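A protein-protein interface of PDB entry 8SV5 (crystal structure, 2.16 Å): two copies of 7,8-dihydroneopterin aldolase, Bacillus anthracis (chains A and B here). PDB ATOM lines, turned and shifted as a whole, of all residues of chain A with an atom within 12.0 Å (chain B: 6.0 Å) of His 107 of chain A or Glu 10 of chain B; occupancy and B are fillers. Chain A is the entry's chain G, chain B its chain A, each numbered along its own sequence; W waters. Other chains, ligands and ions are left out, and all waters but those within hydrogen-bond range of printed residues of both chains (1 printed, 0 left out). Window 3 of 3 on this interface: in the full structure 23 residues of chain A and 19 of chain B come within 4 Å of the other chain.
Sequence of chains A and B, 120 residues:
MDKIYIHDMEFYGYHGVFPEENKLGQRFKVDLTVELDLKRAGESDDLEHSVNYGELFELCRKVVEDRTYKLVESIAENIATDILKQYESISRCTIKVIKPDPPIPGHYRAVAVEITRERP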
ATOM      1  N   LYS A  99     -18.258  -9.170  19.642  1.00  0.00           N
ATOM      2  CA  LYS A  99     -19.151  -8.166  19.075  1.00  0.00           C
ATOM      3  C   LYS A  99     -20.311  -8.912  18.426  1.00  0.00           C
ATOM      4  O   LYS A  99     -20.172  -9.413  17.299  1.00  0.00           O
ATOM      5  CB  LYS A  99     -18.408  -7.327  18.036  1.00  0.00           C
ATOM      6  CG  LYS A  99     -18.687  -5.838  18.120  1.00  0.00           C
ATOM      7  CD  LYS A  99     -17.636  -5.039  17.364  1.00  0.00           C
ATOM      8  CE  LYS A  99     -18.259  -3.869  16.625  1.00  0.00           C
ATOM      9  NZ  LYS A  99     -17.267  -3.143  15.784  1.00  0.00           N
ATOM     10  N   PRO A 100     -21.466  -9.034  19.092  1.00  0.00           N
ATOM     11  CA  PRO A 100     -22.548  -9.858  18.534  1.00  0.00           C
ATOM     12  C   PRO A 100     -23.311  -9.204  17.391  1.00  0.00           C
ATOM     13  O   PRO A 100     -23.887  -9.906  16.552  1.00  0.00           O
ATOM     14  CB  PRO A 100     -23.462 -10.103  19.744  1.00  0.00           C
ATOM     15  CG  PRO A 100     -23.232  -8.924  20.631  1.00  0.00           C
ATOM     16  CD  PRO A 100     -21.791  -8.525  20.439  1.00  0.00           C
ATOM     17  N   ASP A 101     -23.324  -7.873  17.338  1.00  0.00           N
ATOM     18  CA  ASP A 101     -24.153  -7.130  16.388  1.00  0.00           C
ATOM     19  C   ASP A 101     -23.312  -6.128  15.604  1.00  0.00           C
ATOM     20  O   ASP A 101     -23.610  -4.929  15.577  1.00  0.00           O
ATOM     21  CB  ASP A 101     -25.293  -6.422  17.122  1.00  0.00           C
ATOM     22  CG  ASP A 101     -25.906  -7.279  18.214  1.00  0.00           C
ATOM     23  OD1 ASP A 101     -26.097  -8.493  17.989  1.00  0.00           O
ATOM     24  OD2 ASP A 101     -26.200  -6.735  19.301  1.00  0.00           O
ATOM     25  N   PRO A 102     -22.263  -6.590  14.929  1.00  0.00           N
ATOM     26  CA  PRO A 102     -21.411  -5.671  14.166  1.00  0.00           C
ATOM     27  C   PRO A 102     -22.151  -5.129  12.958  1.00  0.00           C
ATOM     28  O   PRO A 102     -23.163  -5.701  12.528  1.00  0.00           O
ATOM     29  CB  PRO A 102     -20.232  -6.557  13.738  1.00  0.00           C
ATOM     30  CG  PRO A 102     -20.785  -7.934  13.707  1.00  0.00           C
ATOM     31  CD  PRO A 102     -21.846  -7.997  14.773  1.00  0.00           C
ATOM     32  N   PRO A 103     -21.675  -4.027  12.380  1.00  0.00           N
ATOM     33  CA  PRO A 103     -22.307  -3.477  11.166  1.00  0.00           C
ATOM     34  C   PRO A 103     -21.801  -4.148   9.897  1.00  0.00           C
ATOM     35  O   PRO A 103     -21.188  -3.522   9.024  1.00  0.00           O
ATOM     36  CB  PRO A 103     -21.923  -1.992  11.250  1.00  0.00           C
ATOM     37  CG  PRO A 103     -20.591  -1.990  11.935  1.00  0.00           C
ATOM     38  CD  PRO A 103     -20.548  -3.197  12.846  1.00  0.00           C
ATOM     39  N   ILE A 104     -22.054  -5.451   9.775  1.00  0.00           N
ATOM     40  CA  ILE A 104     -21.640  -6.236   8.625  1.00  0.00           C
ATOM     41  C   ILE A 104     -22.907  -6.715   7.905  1.00  0.00           C
ATOM     42  O   ILE A 104     -23.640  -7.550   8.451  1.00  0.00           O
ATOM     43  CB  ILE A 104     -20.779  -7.430   9.028  1.00  0.00           C
ATOM     44  CG1 ILE A 104     -19.499  -6.964   9.710  1.00  0.00           C
ATOM     45  CG2 ILE A 104     -20.439  -8.293   7.811  1.00  0.00           C
ATOM     46  CD1 ILE A 104     -18.769  -8.083  10.399  1.00  0.00           C
ATOM     47  N   PRO A 105     -23.185  -6.250   6.683  1.00  0.00           N
ATOM     48  CA  PRO A 105     -24.341  -6.783   5.950  1.00  0.00           C
ATOM     49  C   PRO A 105     -24.212  -8.279   5.710  1.00  0.00           C
ATOM     50  O   PRO A 105     -23.381  -8.719   4.908  1.00  0.00           O
ATOM     51  CB  PRO A 105     -24.331  -5.987   4.637  1.00  0.00           C
ATOM     52  CG  PRO A 105     -23.536  -4.756   4.934  1.00  0.00           C
ATOM     53  CD  PRO A 105     -22.504  -5.173   5.940  1.00  0.00           C
ATOM     54  N   GLY A 106     -25.021  -9.063   6.406  1.00  0.00           N
ATOM     55  CA  GLY A 106     -24.938 -10.506   6.315  1.00  0.00           C
ATOM     56  C   GLY A 106     -25.589 -11.153   7.523  1.00  0.00           C
ATOM     57  O   GLY A 106     -26.266 -10.497   8.315  1.00  0.00           O
ATOM     58  N   HIS A 107     -25.356 -12.459   7.648  1.00  0.00           N
ATOM     59  CA  HIS A 107     -25.996 -13.277   8.672  1.00  0.00           C
ATOM     60  C   HIS A 107     -24.941 -14.120   9.370  1.00  0.00           C
ATOM     61  O   HIS A 107     -24.207 -14.870   8.718  1.00  0.00           O
ATOM     62  CB  HIS A 107     -27.077 -14.162   8.048  1.00  0.00           C
ATOM     63  CG  HIS A 107     -28.073 -13.401   7.230  1.00  0.00           C
ATOM     64  ND1 HIS A 107     -29.322 -13.065   7.702  1.00  0.00           N
ATOM     65  CD2 HIS A 107     -27.993 -12.891   5.979  1.00  0.00           C
ATOM     66  CE1 HIS A 107     -29.974 -12.388   6.772  1.00  0.00           C
ATOM     67  NE2 HIS A 107     -29.189 -12.270   5.716  1.00  0.00           N
ATOM     68  N   TYR A 108     -24.879 -14.003  10.693  1.00  0.00           N
ATOM     69  CA  TYR A 108     -23.842 -14.634  11.500  1.00  0.00           C
ATOM     70  C   TYR A 108     -24.279 -14.530  12.953  1.00  0.00           C
ATOM     71  O   TYR A 108     -25.241 -13.831  13.282  1.00  0.00           O
ATOM     72  CB  TYR A 108     -22.511 -13.911  11.302  1.00  0.00           C
ATOM     73  CG  TYR A 108     -22.698 -12.415  11.259  1.00  0.00           C
ATOM     74  CD1 TYR A 108     -22.877 -11.689  12.427  1.00  0.00           C
ATOM     75  CD2 TYR A 108     -22.735 -11.733  10.051  1.00  0.00           C
ATOM     76  CE1 TYR A 108     -23.066 -10.327  12.397  1.00  0.00           C
ATOM     77  CE2 TYR A 108     -22.923 -10.367  10.011  1.00  0.00           C
ATOM     78  CZ  TYR A 108     -23.089  -9.669  11.187  1.00  0.00           C
ATOM     79  OH  TYR A 108     -23.279  -8.307  11.158  1.00  0.00           O
ATOM     80  N   ARG A 109     -23.552 -15.227  13.825  1.00  0.00           N
ATOM     81  CA  ARG A 109     -23.809 -15.136  15.258  1.00  0.00           C
ATOM     82  C   ARG A 109     -23.045 -13.977  15.892  1.00  0.00           C
ATOM     83  O   ARG A 109     -23.628 -13.170  16.621  1.00  0.00           O
ATOM     84  CB  ARG A 109     -23.441 -16.453  15.950  1.00  0.00           C
ATOM     85  CG  ARG A 109     -23.997 -16.593  17.363  1.00  0.00           C
ATOM     86  CD  ARG A 109     -24.602 -17.976  17.594  1.00  0.00           C
ATOM     87  NE  ARG A 109     -25.789 -18.208  16.778  1.00  0.00           N
ATOM     88  CZ  ARG A 109     -26.741 -19.088  17.062  1.00  0.00           C
ATOM     89  NH1 ARG A 109     -26.685 -19.841  18.149  1.00  0.00           N
ATOM     90  NH2 ARG A 109     -27.776 -19.214  16.236  1.00  0.00           N
ATOM     91  N   ALA A 110     -21.747 -13.875  15.618  1.00  0.00           N
ATOM     92  CA  ALA A 110     -20.927 -12.840  16.230  1.00  0.00           C
ATOM     93  C   ALA A 110     -19.547 -12.862  15.593  1.00  0.00           C
ATOM     94  O   ALA A 110     -19.176 -13.806  14.890  1.00  0.00           O
ATOM     95  CB  ALA A 110     -20.813 -13.048  17.745  1.00  0.00           C
ATOM     96  N   VAL A 111     -18.799 -11.791  15.837  1.00  0.00           N
ATOM     97  CA  VAL A 111     -17.367 -11.739  15.577  1.00  0.00           C
ATOM     98  C   VAL A 111     -16.677 -11.547  16.920  1.00  0.00           C
ATOM     99  O   VAL A 111     -17.267 -11.018  17.869  1.00  0.00           O
ATOM    100  CB  VAL A 111     -16.984 -10.617  14.588  1.00  0.00           C
ATOM    101  CG1 VAL A 111     -17.665 -10.841  13.242  1.00  0.00           C
ATOM    102  CG2 VAL A 111     -17.342  -9.249  15.151  1.00  0.00           C
ATOM    103  N   ASP B   8     -20.576 -18.871  13.213  1.00  0.00           N
ATOM    104  CA  ASP B   8     -21.885 -19.294  12.721  1.00  0.00           C
ATOM    105  C   ASP B   8     -22.393 -18.412  11.586  1.00  0.00           C
ATOM    106  O   ASP B   8     -23.564 -18.027  11.550  1.00  0.00           O
ATOM    107  CB  ASP B   8     -22.902 -19.348  13.868  1.00  0.00           C
ATOM    108  CG  ASP B   8     -23.907 -20.472  13.707  1.00  0.00           C
ATOM    109  OD1 ASP B   8     -23.526 -21.643  13.919  1.00  0.00           O
ATOM    110  OD2 ASP B   8     -25.076 -20.188  13.369  1.00  0.00           O
ATOM    111  N   MET B   9     -21.512 -18.084  10.646  1.00  0.00           N
ATOM    112  CA  MET B   9     -21.964 -17.448   9.417  1.00  0.00           C
ATOM    113  C   MET B   9     -22.981 -18.356   8.740  1.00  0.00           C
ATOM    114  O   MET B   9     -22.815 -19.576   8.712  1.00  0.00           O
ATOM    115  CB  MET B   9     -20.777 -17.236   8.482  1.00  0.00           C
ATOM    116  CG  MET B   9     -19.870 -16.092   8.875  1.00  0.00           C
ATOM    117  SD  MET B   9     -18.406 -16.007   7.827  1.00  0.00           S
ATOM    118  CE  MET B   9     -17.311 -17.117   8.703  1.00  0.00           C
ATOM    119  N   GLU B  10     -24.045 -17.762   8.204  1.00  0.00           N
ATOM    120  CA  GLU B  10     -25.099 -18.514   7.534  1.00  0.00           C
ATOM    121  C   GLU B  10     -25.267 -18.004   6.110  1.00  0.00           C
ATOM    122  O   GLU B  10     -25.394 -16.795   5.888  1.00  0.00           O
ATOM    123  CB  GLU B  10     -26.431 -18.410   8.285  1.00  0.00           C
ATOM    124  CG  GLU B  10     -27.511 -19.329   7.723  1.00  0.00           C
ATOM    125  CD  GLU B  10     -28.828 -19.219   8.466  1.00  0.00           C
ATOM    126  OE1 GLU B  10     -29.013 -19.950   9.462  1.00  0.00           O
ATOM    127  OE2 GLU B  10     -29.679 -18.403   8.052  1.00  0.00           O
ATOM    128  N   PHE B  11     -25.271 -18.935   5.155  1.00  0.00           N
ATOM    129  CA  PHE B  11     -25.471 -18.629   3.749  1.00  0.00           C
ATOM    130  C   PHE B  11     -26.450 -19.633   3.157  1.00  0.00           C
ATOM    131  O   PHE B  11     -26.764 -20.665   3.760  1.00  0.00           O
ATOM    132  CB  PHE B  11     -24.149 -18.694   2.972  1.00  0.00           C
ATOM    133  CG  PHE B  11     -23.019 -17.969   3.640  1.00  0.00           C
ATOM    134  CD1 PHE B  11     -22.924 -16.591   3.564  1.00  0.00           C
ATOM    135  CD2 PHE B  11     -22.052 -18.665   4.345  1.00  0.00           C
ATOM    136  CE1 PHE B  11     -21.884 -15.918   4.182  1.00  0.00           C
ATOM    137  CE2 PHE B  11     -21.012 -17.999   4.962  1.00  0.00           C
ATOM    138  CZ  PHE B  11     -20.927 -16.624   4.880  1.00  0.00           C
ATOM    139  N   TYR B  12     -26.937 -19.322   1.959  1.00  0.00           N
ATOM    140  CA  TYR B  12     -27.701 -20.260   1.150  1.00  0.00           C
ATOM    141  C   TYR B  12     -26.907 -20.563  -0.113  1.00  0.00           C
ATOM    142  O   TYR B  12     -26.522 -19.644  -0.844  1.00  0.00           O
ATOM    143  CB  TYR B  12     -29.072 -19.690   0.788  1.00  0.00           C
ATOM    144  CG  TYR B  12     -30.053 -20.742   0.323  1.00  0.00           C
ATOM    145  CD1 TYR B  12     -30.111 -21.125  -1.013  1.00  0.00           C
ATOM    146  CD2 TYR B  12     -30.916 -21.358   1.218  1.00  0.00           C
ATOM    147  CE1 TYR B  12     -31.005 -22.088  -1.443  1.00  0.00           C
ATOM    148  CE2 TYR B  12     -31.814 -22.325   0.797  1.00  0.00           C
ATOM    149  CZ  TYR B  12     -31.854 -22.686  -0.533  1.00  0.00           C
ATOM    150  OH  TYR B  12     -32.745 -23.647  -0.954  1.00  0.00           O
ATOM    151  N   ARG B  27     -29.191 -24.547   3.285  1.00  0.00           N
ATOM    152  CA  ARG B  27     -28.379 -23.736   4.174  1.00  0.00           C
ATOM    153  C   ARG B  27     -26.948 -24.259   4.217  1.00  0.00           C
ATOM    154  O   ARG B  27     -26.695 -25.463   4.105  1.00  0.00           O
ATOM    155  CB  ARG B  27     -28.935 -23.784   5.594  1.00  0.00           C
ATOM    156  CG  ARG B  27     -30.294 -23.150   5.790  1.00  0.00           C
ATOM    157  CD  ARG B  27     -30.537 -22.935   7.275  1.00  0.00           C
ATOM    158  NE  ARG B  27     -31.898 -22.514   7.577  1.00  0.00           N
ATOM    159  CZ  ARG B  27     -32.929 -23.337   7.697  1.00  0.00           C
ATOM    160  NH1 ARG B  27     -32.802 -24.639   7.495  1.00  0.00           N
ATOM    161  NH2 ARG B  27     -34.120 -22.842   8.027  1.00  0.00           N
ATOM    162  N   PHE B  28     -26.007 -23.338   4.383  1.00  0.00           N
ATOM    163  CA  PHE B  28     -24.639 -23.680   4.740  1.00  0.00           C
ATOM    164  C   PHE B  28     -24.185 -22.709   5.817  1.00  0.00           C
ATOM    165  O   PHE B  28     -24.549 -21.530   5.794  1.00  0.00           O
ATOM    166  CB  PHE B  28     -23.693 -23.603   3.539  1.00  0.00           C
ATOM    167  CG  PHE B  28     -23.952 -24.655   2.505  1.00  0.00           C
ATOM    168  CD1 PHE B  28     -24.965 -24.495   1.574  1.00  0.00           C
ATOM    169  CD2 PHE B  28     -23.192 -25.811   2.469  1.00  0.00           C
ATOM    170  CE1 PHE B  28     -25.212 -25.466   0.624  1.00  0.00           C
ATOM    171  CE2 PHE B  28     -23.435 -26.787   1.521  1.00  0.00           C
ATOM    172  CZ  PHE B  28     -24.446 -26.612   0.598  1.00  0.00           C
ATOM    173  N   LYS B  29     -23.404 -23.212   6.765  1.00  0.00           N
ATOM    174  CA  LYS B  29     -22.864 -22.389   7.835  1.00  0.00           C
ATOM    175  C   LYS B  29     -21.356 -22.568   7.885  1.00  0.00           C
ATOM    176  O   LYS B  29     -20.830 -23.643   7.581  1.00  0.00           O
ATOM    177  CB  LYS B  29     -23.491 -22.753   9.185  1.00  0.00           C
ATOM    178  CG  LYS B  29     -24.942 -22.315   9.331  1.00  0.00           C
ATOM    179  CD  LYS B  29     -25.491 -22.655  10.708  1.00  0.00           C
ATOM    180  CE  LYS B  29     -26.763 -21.877  11.009  1.00  0.00           C
ATOM    181  NZ  LYS B  29     -27.907 -22.775  11.331  1.00  0.00           N
ATOM    182  N   VAL B  30     -20.659 -21.495   8.257  1.00  0.00           N
ATOM    183  CA  VAL B  30     -19.205 -21.499   8.347  1.00  0.00           C
ATOM    184  C   VAL B  30     -18.784 -20.929   9.695  1.00  0.00           C
ATOM    185  O   VAL B  30     -19.311 -19.898  10.135  1.00  0.00           O
ATOM    186  CB  VAL B  30     -18.547 -20.709   7.201  1.00  0.00           C
ATOM    187  CG1 VAL B  30     -17.026 -20.695   7.359  1.00  0.00           C
ATOM    188  CG2 VAL B  30     -18.929 -21.300   5.851  1.00  0.00           C
ATOM    189  N   PHE B  57     -15.509 -11.895   6.366  1.00  0.00           N
ATOM    190  CA  PHE B  57     -16.857 -12.398   6.121  1.00  0.00           C
ATOM    191  C   PHE B  57     -17.162 -12.415   4.630  1.00  0.00           C
ATOM    192  O   PHE B  57     -17.620 -13.428   4.087  1.00  0.00           O
ATOM    193  CB  PHE B  57     -17.891 -11.548   6.858  1.00  0.00           C
ATOM    194  CG  PHE B  57     -19.308 -11.843   6.451  1.00  0.00           C
ATOM    195  CD1 PHE B  57     -20.009 -12.879   7.045  1.00  0.00           C
ATOM    196  CD2 PHE B  57     -19.931 -11.101   5.459  1.00  0.00           C
ATOM    197  CE1 PHE B  57     -21.309 -13.162   6.669  1.00  0.00           C
ATOM    198  CE2 PHE B  57     -21.232 -11.380   5.078  1.00  0.00           C
ATOM    199  CZ  PHE B  57     -21.920 -12.413   5.684  1.00  0.00           C
ATOM    200  N   GLU B  65     -21.508 -18.519  -1.550  1.00  0.00           N
ATOM    201  CA  GLU B  65     -22.642 -18.050  -2.334  1.00  0.00           C
ATOM    202  C   GLU B  65     -22.302 -17.663  -3.767  1.00  0.00           C
ATOM    203  O   GLU B  65     -23.202 -17.670  -4.613  1.00  0.00           O
ATOM    204  CB  GLU B  65     -23.316 -16.851  -1.648  1.00  0.00           C
ATOM    205  CG  GLU B  65     -23.806 -17.151  -0.246  1.00  0.00           C
ATOM    206  CD  GLU B  65     -24.832 -16.148   0.247  1.00  0.00           C
ATOM    207  OE1 GLU B  65     -24.670 -14.942  -0.035  1.00  0.00           O
ATOM    208  OE2 GLU B  65     -25.796 -16.567   0.922  1.00  0.00           O
HETATM  209  O   HOH W   1     -24.740 -14.138   5.229  1.00  0.00           O
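The backbone NH of Glu 10 of chain B is in hydrogen-bond range of the backbone carbonyl oxygen of His 107 of chain A.
The backbone NH (N) of Asp 8 of chain B is in hydrogen-bond range of the backbone carbonyl oxygen (O) of Val 30 of chain B (3.5 Å). N of Met 9 of chain B lies within hydrogen-bond range of O of Val 30 of chain B (2.9 Å). OE1 of Glu 10 of chain B is in salt-bridge range of NZ of Lys 29 of chain B, 3.6 Å away. The backbone carbonyl oxygen (O) of Pro 102 of chain A lies within hydrogen-bond range of the side-chain hydroxyl (OH) of Tyr 108 of chain A (2.9 Å). O of Ile 104 of chain A sits at hydrogen-bond distance from OH of Tyr 108 of chain A, at 2.8 Å.
CG2 of Ile 104 of chain A touches CD2 of Phe 57 of chain B, 3.7 Å away. CE2 of Phe 57 of chain B touches O of Pro 105 of chain A (3.4 Å). Phe 57 of chain B touches Gly 106 of chain A (CZ to CA, 3.6 Å). His 107 of chain A touches Met 9 of chain B. His 107 of chain A touches Phe 57 of chain B. Tyr 108 of chain A touches Asp 8 of chain B. CA of Met 9 of chain B touches CA of Tyr 108 of chain A, at 3.97 Å. CD2 of Tyr 108 of chain A touches CE1 of Phe 57 of chain B (3.9 Å). Arg 109 of chain A touches Asp 8 of chain B (CB to CB, 3.6 Å).
Pro 102 of chain A touches none of the printed residues of chain B. Printed residues of chain B within 4 Å of Pro 105 of chain A: Phe 57 (3.4 Å). Printed residues of chain B within 4 Å of Gly 106 of chain A: Phe 57 (3.6 Å). Of chain B, only Met 9 (3.5 Å), Glu 10 (2.9 Å) and Phe 57 (3.9 Å) come within 4 Å of His 107 of chain A. Of the printed residues of chain B, Tyr 108 of chain A touches Asp 8 (3.4 Å), Met 9 (3.97 Å) and Phe 57 (3.9 Å). Printed residues of chain B within 4 Å of Arg 109 of chain A: Asp 8. Of chain A, only His 107 (2.9 Å) comes within 4 Å of Glu 10 of chain B. No residue of chain A comes within 4 Å of Phe 11 of chain B. No residue of chain A comes within 4 Å of Arg 27 of chain B. Phe 28 of chain B touches none of the printed residues of chain A. No residue of chain A comes within 4 Å of Val 30 of chain B. Of the printed residues of chain A, Phe 57 of chain B touches Ile 104 (3.7 Å), Pro 105 (3.4 Å), Gly 106 (3.6 Å), His 107 (3.9 Å) and Tyr 108 (3.9 Å). The nearest printed residue of chain B that does not touch Ile 104 of chain A is Met 9 of chain B (7.9 Å).
No position is printed for both chains.
Of the 11 printed residues of chain B, 4 touch a printed residue of chain A. Of the 13 printed residues of chain A, 6 touch a printed residue of chain B. Hydrophobic or aromatic side chains of chain A within 4 Å of the printed part of chain B: Ile 104, His 107 and Tyr 108. Among the printed residues, no Asp or Glu carboxylate lies within 4 Å of a Lys or Arg side-chain nitrogen of the other chain.
Water W1 bridges the backbone carbonyl oxygen (O) of Glu 10 of chain B (2.8 Å) and the backbone NH (N) of His 107 of chain A (3.0 Å).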
